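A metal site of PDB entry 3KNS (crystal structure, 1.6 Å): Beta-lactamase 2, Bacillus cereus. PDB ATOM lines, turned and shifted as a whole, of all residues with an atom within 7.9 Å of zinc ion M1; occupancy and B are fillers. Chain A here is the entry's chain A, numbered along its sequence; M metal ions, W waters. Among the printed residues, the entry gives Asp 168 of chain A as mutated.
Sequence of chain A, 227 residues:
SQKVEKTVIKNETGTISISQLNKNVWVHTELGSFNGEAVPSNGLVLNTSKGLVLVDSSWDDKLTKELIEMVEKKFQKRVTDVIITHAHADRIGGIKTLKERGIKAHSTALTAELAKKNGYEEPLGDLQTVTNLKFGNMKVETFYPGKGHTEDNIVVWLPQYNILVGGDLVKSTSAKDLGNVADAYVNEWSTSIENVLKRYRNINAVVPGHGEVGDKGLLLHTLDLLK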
ATOM      1  N   TRP A  59     -10.040   9.734  21.419  1.00  0.00           N
ATOM      2  CA  TRP A  59     -10.255  10.722  22.448  1.00  0.00           C
ATOM      3  C   TRP A  59      -9.478  11.982  22.286  1.00  0.00           C
ATOM      4  O   TRP A  59      -9.884  13.057  22.743  1.00  0.00           O
ATOM      5  CB  TRP A  59      -9.854  10.117  23.776  1.00  0.00           C
ATOM      6  CG  TRP A  59     -10.625   8.938  24.219  1.00  0.00           C
ATOM      7  CD1 TRP A  59     -10.268   7.646  24.115  1.00  0.00           C
ATOM      8  CD2 TRP A  59     -11.874   8.967  24.898  1.00  0.00           C
ATOM      9  NE1 TRP A  59     -11.200   6.839  24.699  1.00  0.00           N
ATOM     10  CE2 TRP A  59     -12.225   7.626  25.157  1.00  0.00           C
ATOM     11  CE3 TRP A  59     -12.713   9.985  25.294  1.00  0.00           C
ATOM     12  CZ2 TRP A  59     -13.351   7.286  25.834  1.00  0.00           C
ATOM     13  CZ3 TRP A  59     -13.890   9.623  25.956  1.00  0.00           C
ATOM     14  CH2 TRP A  59     -14.167   8.298  26.233  1.00  0.00           C
ATOM     15  N   HIS A  86     -20.226  11.877  16.105  1.00  0.00           N
ATOM     16  CA  HIS A  86     -20.739  13.070  16.743  1.00  0.00           C
ATOM     17  C   HIS A  86     -19.586  13.898  17.184  1.00  0.00           C
ATOM     18  O   HIS A  86     -18.437  13.460  17.114  1.00  0.00           O
ATOM     19  CB  HIS A  86     -21.810  12.821  17.842  1.00  0.00           C
ATOM     20  CG  HIS A  86     -21.304  12.290  19.135  1.00  0.00           C
ATOM     21  ND1 HIS A  86     -21.060  10.952  19.345  1.00  0.00           N
ATOM     22  CD2 HIS A  86     -21.071  12.917  20.298  1.00  0.00           C
ATOM     23  CE1 HIS A  86     -20.665  10.797  20.597  1.00  0.00           C
ATOM     24  NE2 HIS A  86     -20.633  11.982  21.184  1.00  0.00           N
ATOM     25  N   ALA A  87     -19.877  15.113  17.635  1.00  0.00           N
ATOM     26  CA  ALA A  87     -18.836  16.103  17.895  1.00  0.00           C
ATOM     27  C   ALA A  87     -18.356  16.117  19.338  1.00  0.00           C
ATOM     28  O   ALA A  87     -18.076  17.209  19.891  1.00  0.00           O
ATOM     29  CB  ALA A  87     -19.278  17.495  17.460  1.00  0.00           C
ATOM     30  N   HIS A  88     -18.091  14.955  19.908  1.00  0.00           N
ATOM     31  CA  HIS A  88     -17.422  14.872  21.200  1.00  0.00           C
ATOM     32  C   HIS A  88     -16.072  14.164  21.052  1.00  0.00           C
ATOM     33  O   HIS A  88     -15.818  13.433  20.092  1.00  0.00           O
ATOM     34  CB  HIS A  88     -18.266  14.029  22.171  1.00  0.00           C
ATOM     35  CG  HIS A  88     -19.476  14.724  22.721  1.00  0.00           C
ATOM     36  ND1 HIS A  88     -20.498  14.011  23.334  1.00  0.00           N
ATOM     37  CD2 HIS A  88     -19.797  16.028  22.798  1.00  0.00           C
ATOM     38  CE1 HIS A  88     -21.394  14.889  23.777  1.00  0.00           C
ATOM     39  NE2 HIS A  88     -21.010  16.109  23.441  1.00  0.00           N
ATOM     40  N   ALA A  89     -15.251  14.266  22.116  1.00  0.00           N
ATOM     41  CA  ALA A  89     -13.850  13.895  22.047  1.00  0.00           C
ATOM     42  C   ALA A  89     -13.611  12.460  21.639  1.00  0.00           C
ATOM     43  O   ALA A  89     -12.680  12.179  20.886  1.00  0.00           O
ATOM     44  CB  ALA A  89     -13.193  14.122  23.415  1.00  0.00           C
ATOM     45  N   ASP A  90     -14.435  11.551  22.134  1.00  0.00           N
ATOM     46  CA  ASP A  90     -14.204  10.169  21.765  1.00  0.00           C
ATOM     47  C   ASP A  90     -14.320   9.865  20.306  1.00  0.00           C
ATOM     48  O   ASP A  90     -13.776   8.862  19.826  1.00  0.00           O
ATOM     49  CB  ASP A  90     -15.021   9.142  22.577  1.00  0.00           C
ATOM     50  CG  ASP A  90     -16.477   9.458  22.729  1.00  0.00           C
ATOM     51  OD1 ASP A  90     -17.000  10.459  22.237  1.00  0.00           O
ATOM     52  OD2 ASP A  90     -17.100   8.604  23.363  1.00  0.00           O
ATOM     53  N   ARG A  91     -15.040  10.725  19.595  1.00  0.00           N
ATOM     54  CA  ARG A  91     -15.257  10.585  18.200  1.00  0.00           C
ATOM     55  C   ARG A  91     -14.398  11.479  17.348  1.00  0.00           C
ATOM     56  O   ARG A  91     -13.833  11.030  16.344  1.00  0.00           O
ATOM     57  CB  ARG A  91     -16.712  10.896  17.910  1.00  0.00           C
ATOM     58  CG  ARG A  91     -17.642  10.164  18.860  1.00  0.00           C
ATOM     59  CD  ARG A  91     -17.528   8.668  18.764  1.00  0.00           C
ATOM     60  NE  ARG A  91     -17.784   8.006  20.011  1.00  0.00           N
ATOM     61  CZ  ARG A  91     -17.536   6.706  20.199  1.00  0.00           C
ATOM     62  NH1 ARG A  91     -17.050   5.985  19.207  1.00  0.00           N
ATOM     63  NH2 ARG A  91     -17.797   6.136  21.346  1.00  0.00           N
ATOM     64  N   HIS A 149     -28.083  10.768  22.156  1.00  0.00           N
ATOM     65  CA  HIS A 149     -26.940  11.075  22.979  1.00  0.00           C
ATOM     66  C   HIS A 149     -26.533  12.542  22.809  1.00  0.00           C
ATOM     67  O   HIS A 149     -26.203  13.269  23.765  1.00  0.00           O
ATOM     68  CB  HIS A 149     -25.794  10.139  22.650  1.00  0.00           C
ATOM     69  CG  HIS A 149     -24.511  10.579  23.221  1.00  0.00           C
ATOM     70  ND1 HIS A 149     -24.214  10.518  24.568  1.00  0.00           N
ATOM     71  CD2 HIS A 149     -23.412  11.088  22.613  1.00  0.00           C
ATOM     72  CE1 HIS A 149     -23.013  11.001  24.754  1.00  0.00           C
ATOM     73  NE2 HIS A 149     -22.510  11.353  23.589  1.00  0.00           N
ATOM     74  N   THR A 150     -26.524  12.991  21.548  1.00  0.00           N
ATOM     75  CA  THR A 150     -26.382  14.371  21.181  1.00  0.00           C
ATOM     76  C   THR A 150     -27.390  14.715  20.115  1.00  0.00           C
ATOM     77  O   THR A 150     -28.056  13.830  19.548  1.00  0.00           O
ATOM     78  CB  THR A 150     -25.014  14.682  20.640  1.00  0.00           C
ATOM     79  OG1 THR A 150     -24.731  13.771  19.575  1.00  0.00           O
ATOM     80  CG2 THR A 150     -23.984  14.534  21.749  1.00  0.00           C
ATOM     81  N   ASP A 152     -26.666  15.519  17.144  1.00  0.00           N
ATOM     82  CA  ASP A 152     -26.112  15.228  15.836  1.00  0.00           C
ATOM     83  C   ASP A 152     -25.700  13.790  15.600  1.00  0.00           C
ATOM     84  O   ASP A 152     -25.369  13.426  14.475  1.00  0.00           O
ATOM     85  CB  ASP A 152     -24.859  16.073  15.615  1.00  0.00           C
ATOM     86  CG  ASP A 152     -23.753  15.787  16.599  1.00  0.00           C
ATOM     87  OD1 ASP A 152     -24.035  15.705  17.802  1.00  0.00           O
ATOM     88  OD2 ASP A 152     -22.581  15.650  16.184  1.00  0.00           O
ATOM     89  N   ASN A 153     -25.768  12.962  16.632  1.00  0.00           N
ATOM     90  CA  ASN A 153     -25.273  11.601  16.505  1.00  0.00           C
ATOM     91  C   ASN A 153     -25.777  10.861  15.288  1.00  0.00           C
ATOM     92  O   ASN A 153     -26.977  10.878  14.986  1.00  0.00           O
ATOM     93  CB  ASN A 153     -25.498  10.809  17.769  1.00  0.00           C
ATOM     94  CG  ASN A 153     -26.930  10.854  18.348  1.00  0.00           C
ATOM     95  OD1 ASN A 153     -27.045  10.701  19.564  1.00  0.00           O
ATOM     96  ND2 ASN A 153     -27.967  11.002  17.531  1.00  0.00           N
ATOM     97  N   GLY A 167     -22.052   4.151  17.825  1.00  0.00           N
ATOM     98  CA  GLY A 167     -21.531   5.203  18.639  1.00  0.00           C
ATOM     99  C   GLY A 167     -22.260   5.325  19.960  1.00  0.00           C
ATOM    100  O   GLY A 167     -22.781   4.363  20.472  1.00  0.00           O
ATOM    101  N   ASP A 168     -22.239   6.505  20.560  1.00  0.00           N
ATOM    102  CA  ASP A 168     -22.726   6.649  21.903  1.00  0.00           C
ATOM    103  C   ASP A 168     -24.250   6.608  21.942  1.00  0.00           C
ATOM    104  O   ASP A 168     -24.804   6.462  23.010  1.00  0.00           O
ATOM    105  CB  ASP A 168     -22.276   7.983  22.541  1.00  0.00           C
ATOM    106  CG  ASP A 168     -20.828   7.987  22.939  1.00  0.00           C
ATOM    107  OD1 ASP A 168     -19.981   7.970  22.040  1.00  0.00           O
ATOM    108  OD2 ASP A 168     -20.578   8.044  24.141  1.00  0.00           O
ATOM    109  N   LEU A 169     -24.890   6.600  20.797  1.00  0.00           N
ATOM    110  CA  LEU A 169     -26.333   6.364  20.725  1.00  0.00           C
ATOM    111  C   LEU A 169     -26.710   4.990  21.237  1.00  0.00           C
ATOM    112  O   LEU A 169     -27.830   4.799  21.689  1.00  0.00           O
ATOM    113  CB  LEU A 169     -26.795   6.504  19.270  1.00  0.00           C
ATOM    114  CG  LEU A 169     -28.298   6.539  19.037  1.00  0.00           C
ATOM    115  CD1 LEU A 169     -28.932   7.861  19.497  1.00  0.00           C
ATOM    116  CD2 LEU A 169     -28.566   6.268  17.571  1.00  0.00           C
ATOM    117  N   LYS A 171     -25.848   1.690  23.610  1.00  0.00           N
ATOM    118  CA  LYS A 171     -25.197   1.172  24.764  1.00  0.00           C
ATOM    119  C   LYS A 171     -24.937  -0.290  24.696  1.00  0.00           C
ATOM    120  O   LYS A 171     -25.688  -1.024  24.078  1.00  0.00           O
ATOM    121  CB  LYS A 171     -26.039   1.446  25.998  1.00  0.00           C
ATOM    122  CG  LYS A 171     -26.356   2.889  26.202  1.00  0.00           C
ATOM    123  CD  LYS A 171     -25.201   3.772  25.994  1.00  0.00           C
ATOM    124  CE  LYS A 171     -25.557   5.184  26.166  1.00  0.00           C
ATOM    125  NZ  LYS A 171     -24.373   6.051  25.903  1.00  0.00           N
ATOM    126  N   ASN A 180     -23.512  10.942  30.128  1.00  0.00           N
ATOM    127  CA  ASN A 180     -23.782  12.333  30.230  1.00  0.00           C
ATOM    128  C   ASN A 180     -24.964  12.730  29.362  1.00  0.00           C
ATOM    129  O   ASN A 180     -24.943  12.521  28.156  1.00  0.00           O
ATOM    130  CB  ASN A 180     -22.536  13.102  29.804  1.00  0.00           C
ATOM    131  CG  ASN A 180     -22.660  14.558  29.997  1.00  0.00           C
ATOM    132  OD1 ASN A 180     -23.680  15.151  29.697  1.00  0.00           O
ATOM    133  ND2 ASN A 180     -21.570  15.191  30.448  1.00  0.00           N
ATOM    134  N   HIS A 210     -19.123   2.359  23.304  1.00  0.00           N
ATOM    135  CA  HIS A 210     -18.278   1.877  24.357  1.00  0.00           C
ATOM    136  C   HIS A 210     -18.764   0.524  24.774  1.00  0.00           C
ATOM    137  O   HIS A 210     -19.954   0.306  24.924  1.00  0.00           O
ATOM    138  CB  HIS A 210     -18.432   2.798  25.565  1.00  0.00           C
ATOM    139  CG  HIS A 210     -18.146   4.222  25.262  1.00  0.00           C
ATOM    140  ND1 HIS A 210     -16.868   4.739  25.277  1.00  0.00           N
ATOM    141  CD2 HIS A 210     -18.967   5.242  24.903  1.00  0.00           C
ATOM    142  CE1 HIS A 210     -16.921   6.013  24.948  1.00  0.00           C
ATOM    143  NE2 HIS A 210     -18.179   6.340  24.711  1.00  0.00           N
HETATM  144 ZN    ZN M   1     -20.708  12.126  23.286  1.00  0.00          ZN
HETATM  145 ZN    ZN M   2     -18.676   8.232  24.355  1.00  0.00          ZN
HETATM  146  O   HOH W   1     -20.483  12.326  25.621  1.00  0.00           O
HETATM  147  O   HOH W   2     -19.069  11.013  23.685  1.00  0.00           O
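The backbone NH (N) of His 149 sits at hydrogen-bond distance from the side-chain amide oxygen (OD1) of Asn 153 (2.8 Å).
Within 4 Å of zinc ion M1: His 86, His 88 and His 149. The nearest printed residue that does not touch zinc ion M1 is Asp 168 (4.2 Å).
Zinc ion M1 is bound by ND1 of His 88, NE2 of His 149, water W2, NE2 of His 86 and water W1.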
